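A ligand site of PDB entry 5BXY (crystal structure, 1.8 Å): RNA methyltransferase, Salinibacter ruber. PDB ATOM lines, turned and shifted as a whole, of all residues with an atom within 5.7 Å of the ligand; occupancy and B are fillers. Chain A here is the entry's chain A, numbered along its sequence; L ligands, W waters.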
ATOM      1  N   VAL A   3     -18.192  14.873 -23.273  1.00  0.00           N
ATOM      2  CA  VAL A   3     -18.716  15.110 -21.920  1.00  0.00           C
ATOM      3  C   VAL A   3     -17.621  15.763 -21.054  1.00  0.00           C
ATOM      4  O   VAL A   3     -16.577  15.141 -20.814  1.00  0.00           O
ATOM      5  CB  VAL A   3     -19.210  13.811 -21.227  1.00  0.00           C
ATOM      6  CG1 VAL A   3     -19.940  14.136 -19.920  1.00  0.00           C
ATOM      7  CG2 VAL A   3     -20.109  13.008 -22.138  1.00  0.00           C
ATOM      8  N   PRO A   4     -17.851  17.007 -20.580  1.00  0.00           N
ATOM      9  CA  PRO A   4     -16.808  17.685 -19.818  1.00  0.00           C
ATOM     10  C   PRO A   4     -16.704  17.131 -18.396  1.00  0.00           C
ATOM     11  O   PRO A   4     -17.681  16.586 -17.904  1.00  0.00           O
ATOM     12  CB  PRO A   4     -17.301  19.128 -19.774  1.00  0.00           C
ATOM     13  CG  PRO A   4     -18.786  19.023 -19.794  1.00  0.00           C
ATOM     14  CD  PRO A   4     -19.082  17.828 -20.679  1.00  0.00           C
ATOM     15  N   TYR A   5     -15.545  17.305 -17.750  1.00  0.00           N
ATOM     16  CA  TYR A   5     -15.450  17.057 -16.297  1.00  0.00           C
ATOM     17  C   TYR A   5     -15.998  18.244 -15.486  1.00  0.00           C
ATOM     18  O   TYR A   5     -15.251  19.196 -15.156  1.00  0.00           O
ATOM     19  CB  TYR A   5     -14.025  16.673 -15.823  1.00  0.00           C
ATOM     20  CG  TYR A   5     -13.996  16.516 -14.327  1.00  0.00           C
ATOM     21  CD1 TYR A   5     -14.786  15.565 -13.696  1.00  0.00           C
ATOM     22  CD2 TYR A   5     -13.253  17.388 -13.510  1.00  0.00           C
ATOM     23  CE1 TYR A   5     -14.807  15.446 -12.309  1.00  0.00           C
ATOM     24  CE2 TYR A   5     -13.272  17.281 -12.114  1.00  0.00           C
ATOM     25  CZ  TYR A   5     -14.048  16.300 -11.519  1.00  0.00           C
ATOM     26  OH  TYR A   5     -14.091  16.175 -10.152  1.00  0.00           O
ATOM     27  N   VAL A   6     -17.280  18.182 -15.180  1.00  0.00           N
ATOM     28  CA  VAL A   6     -17.922  19.034 -14.156  1.00  0.00           C
ATOM     29  C   VAL A   6     -18.714  18.062 -13.287  1.00  0.00           C
ATOM     30  O   VAL A   6     -19.608  17.399 -13.808  1.00  0.00           O
ATOM     31  CB  VAL A   6     -18.877  20.088 -14.756  1.00  0.00           C
ATOM     32  CG1 VAL A   6     -19.587  20.867 -13.648  1.00  0.00           C
ATOM     33  CG2 VAL A   6     -18.121  21.033 -15.683  1.00  0.00           C
ATOM     34  N   PRO A   7     -18.339  17.925 -11.981  1.00  0.00           N
ATOM     35  CA  PRO A   7     -18.892  16.855 -11.176  1.00  0.00           C
ATOM     36  C   PRO A   7     -20.305  17.128 -10.683  1.00  0.00           C
ATOM     37  O   PRO A   7     -20.729  18.275 -10.619  1.00  0.00           O
ATOM     38  CB  PRO A   7     -17.888  16.759  -9.996  1.00  0.00           C
ATOM     39  CG  PRO A   7     -17.294  18.092  -9.897  1.00  0.00           C
ATOM     40  CD  PRO A   7     -17.198  18.565 -11.314  1.00  0.00           C
ATOM     41  N   THR A   8     -20.976  16.059 -10.282  1.00  0.00           N
ATOM     42  CA  THR A   8     -22.253  16.164  -9.595  1.00  0.00           C
ATOM     43  C   THR A   8     -21.989  16.683  -8.165  1.00  0.00           C
ATOM     44  O   THR A   8     -21.153  16.122  -7.458  1.00  0.00           O
ATOM     45  CB  THR A   8     -22.941  14.780  -9.529  1.00  0.00           C
ATOM     46  OG1 THR A   8     -23.191  14.334 -10.859  1.00  0.00           O
ATOM     47  CG2 THR A   8     -24.246  14.854  -8.785  1.00  0.00           C
ATOM     48  N   VAL A  13     -25.392  13.708  -5.308  1.00  0.00           N
ATOM     49  CA  VAL A  13     -24.908  12.317  -5.267  1.00  0.00           C
ATOM     50  C   VAL A  13     -25.671  11.542  -4.205  1.00  0.00           C
ATOM     51  O   VAL A  13     -26.158  10.438  -4.451  1.00  0.00           O
ATOM     52  CB  VAL A  13     -23.381  12.207  -5.025  1.00  0.00           C
ATOM     53  CG1 VAL A  13     -22.946  10.756  -4.865  1.00  0.00           C
ATOM     54  CG2 VAL A  13     -22.605  12.868  -6.156  1.00  0.00           C
ATOM     55  N   ASP A  30     -20.325   3.528 -12.042  1.00  0.00           N
ATOM     56  CA  ASP A  30     -20.479   4.907 -12.443  1.00  0.00           C
ATOM     57  C   ASP A  30     -19.749   5.040 -13.792  1.00  0.00           C
ATOM     58  O   ASP A  30     -18.518   4.836 -13.879  1.00  0.00           O
ATOM     59  CB  ASP A  30     -19.958   5.888 -11.401  1.00  0.00           C
ATOM     60  CG  ASP A  30     -20.243   7.343 -11.788  1.00  0.00           C
ATOM     61  OD1 ASP A  30     -21.210   7.625 -12.551  1.00  0.00           O
ATOM     62  OD2 ASP A  30     -19.520   8.236 -11.291  1.00  0.00           O
ATOM     63  N   LEU A  31     -20.535   5.309 -14.826  1.00  0.00           N
ATOM     64  CA  LEU A  31     -20.036   5.390 -16.193  1.00  0.00           C
ATOM     65  C   LEU A  31     -19.649   6.823 -16.523  1.00  0.00           C
ATOM     66  O   LEU A  31     -20.525   7.689 -16.677  1.00  0.00           O
ATOM     67  CB  LEU A  31     -21.093   4.847 -17.168  1.00  0.00           C
ATOM     68  CG  LEU A  31     -21.592   3.421 -16.871  1.00  0.00           C
ATOM     69  CD1 LEU A  31     -22.529   2.917 -17.958  1.00  0.00           C
ATOM     70  CD2 LEU A  31     -20.443   2.421 -16.669  1.00  0.00           C
ATOM     71  N   GLY A  32     -18.327   7.068 -16.566  1.00  0.00           N
ATOM     72  CA  GLY A  32     -17.761   8.425 -16.610  1.00  0.00           C
ATOM     73  C   GLY A  32     -17.582   8.907 -15.168  1.00  0.00           C
ATOM     74  O   GLY A  32     -18.247   9.838 -14.722  1.00  0.00           O
ATOM     75  N   SER A  33     -16.662   8.272 -14.451  1.00  0.00           N
ATOM     76  CA  SER A  33     -16.618   8.390 -12.985  1.00  0.00           C
ATOM     77  C   SER A  33     -15.921   9.624 -12.418  1.00  0.00           C
ATOM     78  O   SER A  33     -16.056   9.895 -11.215  1.00  0.00           O
ATOM     79  CB  SER A  33     -16.073   7.087 -12.339  1.00  0.00           C
ATOM     80  OG  SER A  33     -14.834   6.701 -12.893  1.00  0.00           O
ATOM     81  N   GLY A  34     -15.172  10.373 -13.243  1.00  0.00           N
ATOM     82  CA  GLY A  34     -14.597  11.641 -12.781  1.00  0.00           C
ATOM     83  C   GLY A  34     -13.652  11.507 -11.585  1.00  0.00           C
ATOM     84  O   GLY A  34     -12.763  10.649 -11.600  1.00  0.00           O
ATOM     85  N   ASP A  35     -13.876  12.298 -10.529  1.00  0.00           N
ATOM     86  CA  ASP A  35     -13.051  12.189  -9.317  1.00  0.00           C
ATOM     87  C   ASP A  35     -13.419  11.032  -8.383  1.00  0.00           C
ATOM     88  O   ASP A  35     -12.858  10.924  -7.275  1.00  0.00           O
ATOM     89  CB  ASP A  35     -12.998  13.517  -8.543  1.00  0.00           C
ATOM     90  CG  ASP A  35     -14.257  13.822  -7.696  1.00  0.00           C
ATOM     91  OD1 ASP A  35     -15.317  13.166  -7.854  1.00  0.00           O
ATOM     92  OD2 ASP A  35     -14.172  14.793  -6.887  1.00  0.00           O
ATOM     93  N   ARG A  37     -16.401  10.370  -6.878  1.00  0.00           N
ATOM     94  CA  ARG A  37     -17.282  10.674  -5.748  1.00  0.00           C
ATOM     95  C   ARG A  37     -18.516   9.789  -5.638  1.00  0.00           C
ATOM     96  O   ARG A  37     -18.943   9.488  -4.522  1.00  0.00           O
ATOM     97  CB  ARG A  37     -17.689  12.149  -5.733  1.00  0.00           C
ATOM     98  CG  ARG A  37     -18.524  12.549  -6.953  1.00  0.00           C
ATOM     99  CD  ARG A  37     -18.834  14.037  -6.958  1.00  0.00           C
ATOM    100  NE  ARG A  37     -17.598  14.821  -6.869  1.00  0.00           N
ATOM    101  CZ  ARG A  37     -17.515  16.114  -6.543  1.00  0.00           C
ATOM    102  NH1 ARG A  37     -18.609  16.837  -6.319  1.00  0.00           N
ATOM    103  NH2 ARG A  37     -16.322  16.684  -6.489  1.00  0.00           N
ATOM    104  N   ILE A  38     -19.095   9.351  -6.762  1.00  0.00           N
ATOM    105  CA  ILE A  38     -20.308   8.541  -6.670  1.00  0.00           C
ATOM    106  C   ILE A  38     -19.987   7.169  -6.091  1.00  0.00           C
ATOM    107  O   ILE A  38     -20.646   6.704  -5.137  1.00  0.00           O
ATOM    108  CB  ILE A  38     -21.071   8.441  -8.020  1.00  0.00           C
ATOM    109  CG1 ILE A  38     -21.421   9.858  -8.521  1.00  0.00           C
ATOM    110  CG2 ILE A  38     -22.303   7.570  -7.872  1.00  0.00           C
ATOM    111  CD1 ILE A  38     -22.296   9.939  -9.731  1.00  0.00           C
ATOM    112  N   ILE A  53     -15.736   3.790 -14.380  1.00  0.00           N
ATOM    113  CA  ILE A  53     -15.106   3.742 -15.698  1.00  0.00           C
ATOM    114  C   ILE A  53     -14.855   5.195 -16.112  1.00  0.00           C
ATOM    115  O   ILE A  53     -15.793   6.009 -16.120  1.00  0.00           O
ATOM    116  CB  ILE A  53     -16.016   3.075 -16.778  1.00  0.00           C
ATOM    117  CG1 ILE A  53     -16.554   1.716 -16.337  1.00  0.00           C
ATOM    118  CG2 ILE A  53     -15.286   2.964 -18.095  1.00  0.00           C
ATOM    119  CD1 ILE A  53     -15.518   0.683 -15.986  1.00  0.00           C
ATOM    120  N   GLU A  54     -13.628   5.510 -16.469  1.00  0.00           N
ATOM    121  CA  GLU A  54     -13.228   6.891 -16.796  1.00  0.00           C
ATOM    122  C   GLU A  54     -12.157   6.933 -17.867  1.00  0.00           C
ATOM    123  O   GLU A  54     -11.162   6.225 -17.789  1.00  0.00           O
ATOM    124  CB  GLU A  54     -12.775   7.622 -15.537  1.00  0.00           C
ATOM    125  CG  GLU A  54     -12.100   8.975 -15.731  1.00  0.00           C
ATOM    126  CD  GLU A  54     -12.999  10.012 -16.372  1.00  0.00           C
ATOM    127  OE1 GLU A  54     -14.109  10.271 -15.827  1.00  0.00           O
ATOM    128  OE2 GLU A  54     -12.595  10.606 -17.406  1.00  0.00           O
ATOM    129  N   ILE A  55     -12.379   7.775 -18.871  1.00  0.00           N
ATOM    130  CA  ILE A  55     -11.479   7.823 -20.045  1.00  0.00           C
ATOM    131  C   ILE A  55     -10.182   8.628 -19.787  1.00  0.00           C
ATOM    132  O   ILE A  55      -9.147   8.326 -20.372  1.00  0.00           O
ATOM    133  CB  ILE A  55     -12.233   8.335 -21.300  1.00  0.00           C
ATOM    134  CG1 ILE A  55     -11.442   8.117 -22.618  1.00  0.00           C
ATOM    135  CG2 ILE A  55     -12.574   9.814 -21.207  1.00  0.00           C
ATOM    136  CD1 ILE A  55     -11.444   6.695 -23.082  1.00  0.00           C
ATOM    137  N   ASP A  56     -10.266   9.645 -18.928  1.00  0.00           N
ATOM    138  CA  ASP A  56      -9.131  10.563 -18.680  1.00  0.00           C
ATOM    139  C   ASP A  56      -8.203   9.986 -17.611  1.00  0.00           C
ATOM    140  O   ASP A  56      -8.622   9.833 -16.460  1.00  0.00           O
ATOM    141  CB  ASP A  56      -9.677  11.919 -18.215  1.00  0.00           C
ATOM    142  CG  ASP A  56      -8.624  13.011 -18.161  1.00  0.00           C
ATOM    143  OD1 ASP A  56      -7.430  12.707 -18.006  1.00  0.00           O
ATOM    144  OD2 ASP A  56      -9.008  14.203 -18.263  1.00  0.00           O
ATOM    145  N   LEU A  59      -7.922  11.827 -14.193  1.00  0.00           N
ATOM    146  CA  LEU A  59      -9.059  11.643 -13.293  1.00  0.00           C
ATOM    147  C   LEU A  59      -9.079  10.259 -12.669  1.00  0.00           C
ATOM    148  O   LEU A  59      -9.429  10.129 -11.509  1.00  0.00           O
ATOM    149  CB  LEU A  59     -10.379  11.965 -14.014  1.00  0.00           C
ATOM    150  CG  LEU A  59     -10.542  13.454 -14.319  1.00  0.00           C
ATOM    151  CD1 LEU A  59     -11.670  13.718 -15.294  1.00  0.00           C
ATOM    152  CD2 LEU A  59     -10.762  14.243 -13.039  1.00  0.00           C
ATOM    153  N   GLY A  81     -10.784   3.702 -19.365  1.00  0.00           N
ATOM    154  CA  GLY A  81     -11.325   3.242 -20.630  1.00  0.00           C
ATOM    155  C   GLY A  81     -12.556   4.007 -21.076  1.00  0.00           C
ATOM    156  O   GLY A  81     -13.073   4.886 -20.365  1.00  0.00           O
ATOM    157  N   ASP A  82     -13.019   3.662 -22.265  1.00  0.00           N
ATOM    158  CA  ASP A  82     -14.224   4.253 -22.836  1.00  0.00           C
ATOM    159  C   ASP A  82     -15.435   3.477 -22.315  1.00  0.00           C
ATOM    160  O   ASP A  82     -15.517   2.236 -22.492  1.00  0.00           O
ATOM    161  CB  ASP A  82     -14.087   4.168 -24.360  1.00  0.00           C
ATOM    162  CG  ASP A  82     -15.282   4.726 -25.129  1.00  0.00           C
ATOM    163  OD1 ASP A  82     -16.316   5.139 -24.566  1.00  0.00           O
ATOM    164  OD2 ASP A  82     -15.128   4.692 -26.384  1.00  0.00           O
ATOM    165  N   LEU A  83     -16.400   4.175 -21.708  1.00  0.00           N
ATOM    166  CA  LEU A  83     -17.601   3.527 -21.164  1.00  0.00           C
ATOM    167  C   LEU A  83     -18.428   2.801 -22.210  1.00  0.00           C
ATOM    168  O   LEU A  83     -19.086   1.803 -21.907  1.00  0.00           O
ATOM    169  CB  LEU A  83     -18.447   4.520 -20.372  1.00  0.00           C
ATOM    170  CG  LEU A  83     -19.184   5.648 -21.145  1.00  0.00           C
ATOM    171  CD1 LEU A  83     -20.570   5.190 -21.556  1.00  0.00           C
ATOM    172  CD2 LEU A  83     -19.284   6.908 -20.302  1.00  0.00           C
ATOM    173  N   PHE A  84     -18.355   3.242 -23.469  1.00  0.00           N
ATOM    174  CA  PHE A  84     -19.054   2.544 -24.574  1.00  0.00           C
ATOM    175  C   PHE A  84     -18.441   1.205 -24.966  1.00  0.00           C
ATOM    176  O   PHE A  84     -19.045   0.453 -25.731  1.00  0.00           O
ATOM    177  CB  PHE A  84     -19.149   3.446 -25.798  1.00  0.00           C
ATOM    178  CG  PHE A  84     -20.116   4.572 -25.632  1.00  0.00           C
ATOM    179  CD1 PHE A  84     -21.445   4.295 -25.783  1.00  0.00           C
ATOM    180  CD2 PHE A  84     -19.719   5.866 -25.363  1.00  0.00           C
ATOM    181  CE1 PHE A  84     -22.394   5.268 -25.664  1.00  0.00           C
ATOM    182  CE2 PHE A  84     -20.684   6.870 -25.221  1.00  0.00           C
ATOM    183  CZ  PHE A  84     -22.021   6.548 -25.394  1.00  0.00           C
ATOM    184  N   LEU A  96     -25.136   7.795 -13.855  1.00  0.00           N
ATOM    185  CA  LEU A  96     -24.743   8.525 -15.058  1.00  0.00           C
ATOM    186  C   LEU A  96     -24.854  10.038 -14.849  1.00  0.00           C
ATOM    187  O   LEU A  96     -25.886  10.512 -14.369  1.00  0.00           O
ATOM    188  CB  LEU A  96     -25.659   8.175 -16.236  1.00  0.00           C
ATOM    189  CG  LEU A  96     -25.896   6.717 -16.612  1.00  0.00           C
ATOM    190  CD1 LEU A  96     -26.967   6.612 -17.667  1.00  0.00           C
ATOM    191  CD2 LEU A  96     -24.594   6.096 -17.083  1.00  0.00           C
ATOM    192  N   TYR A  97     -23.821  10.782 -15.224  1.00  0.00           N
ATOM    193  CA  TYR A  97     -23.970  12.238 -15.472  1.00  0.00           C
ATOM    194  C   TYR A  97     -23.197  12.591 -16.727  1.00  0.00           C
ATOM    195  O   TYR A  97     -22.008  12.935 -16.672  1.00  0.00           O
ATOM    196  CB  TYR A  97     -23.494  13.051 -14.296  1.00  0.00           C
ATOM    197  CG  TYR A  97     -23.642  14.557 -14.425  1.00  0.00           C
ATOM    198  CD1 TYR A  97     -24.718  15.139 -15.135  1.00  0.00           C
ATOM    199  CD2 TYR A  97     -22.742  15.393 -13.800  1.00  0.00           C
ATOM    200  CE1 TYR A  97     -24.857  16.536 -15.192  1.00  0.00           C
ATOM    201  CE2 TYR A  97     -22.865  16.774 -13.855  1.00  0.00           C
ATOM    202  CZ  TYR A  97     -23.922  17.339 -14.549  1.00  0.00           C
ATOM    203  OH  TYR A  97     -23.999  18.728 -14.581  1.00  0.00           O
ATOM    204  N   LEU A  98     -23.894  12.478 -17.857  1.00  0.00           N
ATOM    205  CA  LEU A  98     -23.232  12.548 -19.157  1.00  0.00           C
ATOM    206  C   LEU A  98     -23.837  13.711 -19.966  1.00  0.00           C
ATOM    207  O   LEU A  98     -23.607  14.864 -19.604  1.00  0.00           O
ATOM    208  CB  LEU A  98     -23.305  11.175 -19.850  1.00  0.00           C
ATOM    209  CG  LEU A  98     -22.543  10.057 -19.107  1.00  0.00           C
ATOM    210  CD1 LEU A  98     -22.898   8.690 -19.703  1.00  0.00           C
ATOM    211  CD2 LEU A  98     -21.047  10.281 -19.153  1.00  0.00           C
ATOM    212  N   HIS A 123     -28.275  11.996 -13.575  1.00  0.00           N
ATOM    213  CA  HIS A 123     -28.312  13.393 -13.182  1.00  0.00           C
ATOM    214  C   HIS A 123     -28.628  14.239 -14.433  1.00  0.00           C
ATOM    215  O   HIS A 123     -27.919  14.178 -15.424  1.00  0.00           O
ATOM    216  CB  HIS A 123     -26.975  13.768 -12.569  1.00  0.00           C
ATOM    217  CG  HIS A 123     -26.834  15.198 -12.153  1.00  0.00           C
ATOM    218  ND1 HIS A 123     -25.619  15.774 -11.911  1.00  0.00           N
ATOM    219  CD2 HIS A 123     -27.756  16.175 -11.957  1.00  0.00           C
ATOM    220  CE1 HIS A 123     -25.782  17.044 -11.566  1.00  0.00           C
ATOM    221  NE2 HIS A 123     -27.076  17.306 -11.597  1.00  0.00           N
HETATM  222  N1  LIG L   1     -19.891  10.738 -12.687  1.00  0.00           N
HETATM  223  C1  LIG L   1     -19.070  11.854 -12.125  1.00  0.00           C
HETATM  224  C2  LIG L   1     -18.344  12.694 -13.198  1.00  0.00           C
HETATM  225  C3  LIG L   1     -19.251  13.350 -14.255  1.00  0.00           C
HETATM  226  S1  LIG L   1     -18.332  14.409 -15.353  1.00  0.00           S
HETATM  227  C4  LIG L   1     -19.975  12.751 -11.314  1.00  0.00           C
HETATM  228  O1  LIG L   1     -19.506  13.572 -10.514  1.00  0.00           O
HETATM  229  O2  LIG L   1     -21.192  12.692 -11.477  1.00  0.00           O
HETATM  230  C5  LIG L   1     -18.240  13.358 -16.788  1.00  0.00           C
HETATM  231  C6  LIG L   1     -17.025  12.408 -16.843  1.00  0.00           C
HETATM  232  O3  LIG L   1     -17.121  11.489 -17.946  1.00  0.00           O
HETATM  233  C7  LIG L   1     -15.694  13.127 -17.050  1.00  0.00           C
HETATM  234  O4  LIG L   1     -14.790  12.840 -15.973  1.00  0.00           O
HETATM  235  C8  LIG L   1     -15.188  12.647 -18.411  1.00  0.00           C
HETATM  236  O5  LIG L   1     -13.753  12.582 -18.554  1.00  0.00           O
HETATM  237  C9  LIG L   1     -15.817  11.274 -18.520  1.00  0.00           C
HETATM  238  N2  LIG L   1     -16.025  10.705 -19.873  1.00  0.00           N
HETATM  239  C10 LIG L   1     -16.407  11.347 -20.986  1.00  0.00           C
HETATM  240  N3  LIG L   1     -16.557  10.545 -22.022  1.00  0.00           N
HETATM  241  C11 LIG L   1     -16.239   9.300 -21.526  1.00  0.00           C
HETATM  242  C12 LIG L   1     -16.220   8.019 -22.120  1.00  0.00           C
HETATM  243  N4  LIG L   1     -16.526   7.830 -23.428  1.00  0.00           N
HETATM  244  N5  LIG L   1     -15.846   6.959 -21.335  1.00  0.00           N
HETATM  245  C13 LIG L   1     -15.540   7.175 -20.036  1.00  0.00           C
HETATM  246  N6  LIG L   1     -15.530   8.352 -19.394  1.00  0.00           N
HETATM  247  C14 LIG L   1     -15.914   9.386 -20.190  1.00  0.00           C
HETATM  248  O   HOH W   1     -21.375   9.608 -14.918  1.00  0.00           O
HETATM  249  O   HOH W   2     -17.292   9.322 -25.809  1.00  0.00           O
HETATM  250  O   HOH W   3     -12.051  14.812 -18.687  1.00  0.00           O
HETATM  251  O   HOH W   4     -17.195  12.295 -24.111  1.00  0.00           O
HETATM  252  O   HOH W   5     -16.732  13.355 -10.255  1.00  0.00           O
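Water W5 lies within hydrogen-bond range of the side-chain carboxylate of Asp 35 and an oxygen (O1) of the ligand.
Water W4 bridges N3 of the ligand and N of Val 3.
Water W3 lies within hydrogen-bond range of O5 of the ligand and OD2 of Asp 56.
The side-chain carboxylate (OE2) of Glu 54 is in hydrogen-bond range of an oxygen (O5) of the ligand, 2.6 Å away.
The backbone NH of Thr 8 is in hydrogen-bond range of an oxygen (O1) of the ligand (2.9 Å).
OG1 of Thr 8 is in hydrogen-bond range of O2 of the ligand (2.7 Å).
A nitrogen (N1) of the ligand lies within hydrogen-bond range of the backbone carbonyl oxygen of Gly 32 (2.8 Å).
N of Leu 83 lies within hydrogen-bond range of N5 of the ligand, at 2.9 Å.
A nitrogen (N1) of the ligand lies within salt-bridge range of the side-chain carboxylate of Asp 30, at 2.9 Å.
A nitrogen (N4) of the ligand sits at hydrogen-bond distance from the side-chain carboxylate (OD1) of Asp 82 (2.9 Å).
A nitrogen (N6) of the ligand is in hydrogen-bond range of the backbone NH (N) of Ile 55.
A sulfur (S1) of the ligand sits close to the backbone carbonyl oxygen (O) of Pro 4.
The backbone carbonyl oxygen (O) of Val 6 sits close to a sulfur (S1) of the ligand (3.6 Å).
Merely in contact with the ligand: Val 3 (3.6 Å), Tyr 5 (3.6 Å), Pro 7 (3.4 Å), Ser 33 (3.7 Å), Gly 34 (3.4 Å), Arg 37 (3.6 Å), Ile 38 (3.4 Å), Leu 59 (3.3 Å), Gly 81 (3.4 Å) and Tyr 97 (3.7 Å).
Hydrophobic or aromatic side chains within 4 Å of the ligand: Val 3, Tyr 5, Pro 7, Ile 38, Ile 55, Leu 59, Leu 83 and Tyr 97.
Within 4 Å of the ligand: Val 3, Pro 4, Tyr 5, Val 6, Pro 7, Thr 8, Asp 30, Gly 32, Ser 33, Gly 34, Arg 37, Ile 38, Glu 54, Ile 55, Leu 59, Gly 81, Asp 82, Leu 83 and Tyr 97.
The backbone NH (N) of Gly 34 is in hydrogen-bond range of the side-chain carboxylate (OE1) of Glu 54 (2.8 Å).
The backbone carbonyl oxygen of Thr 8 sits at hydrogen-bond distance from the guanidinium group of Arg 37, 2.9 Å away.
The side-chain hydroxyl of Thr 8 sits at hydrogen-bond distance from a ring nitrogen (ND1) of His 123, 3.0 Å away.
The backbone NH (N) of Gly 32 sits at hydrogen-bond distance from the backbone carbonyl oxygen (O) of Ile 53 (2.8 Å).
The backbone carbonyl oxygen (O) of Asp 30 sits at hydrogen-bond distance from the backbone NH (N) of Ile 53, 3.0 Å away.
The side-chain carboxylate (OD1) of Asp 82 is in hydrogen-bond range of the backbone NH (N) of Phe 84, 3.0 Å away.
N of Ile 55 sits at hydrogen-bond distance from O of Gly 81 (3.3 Å).
The backbone NH of Ser 33 is in hydrogen-bond range of the backbone carbonyl oxygen of Ile 53, 2.9 Å away.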
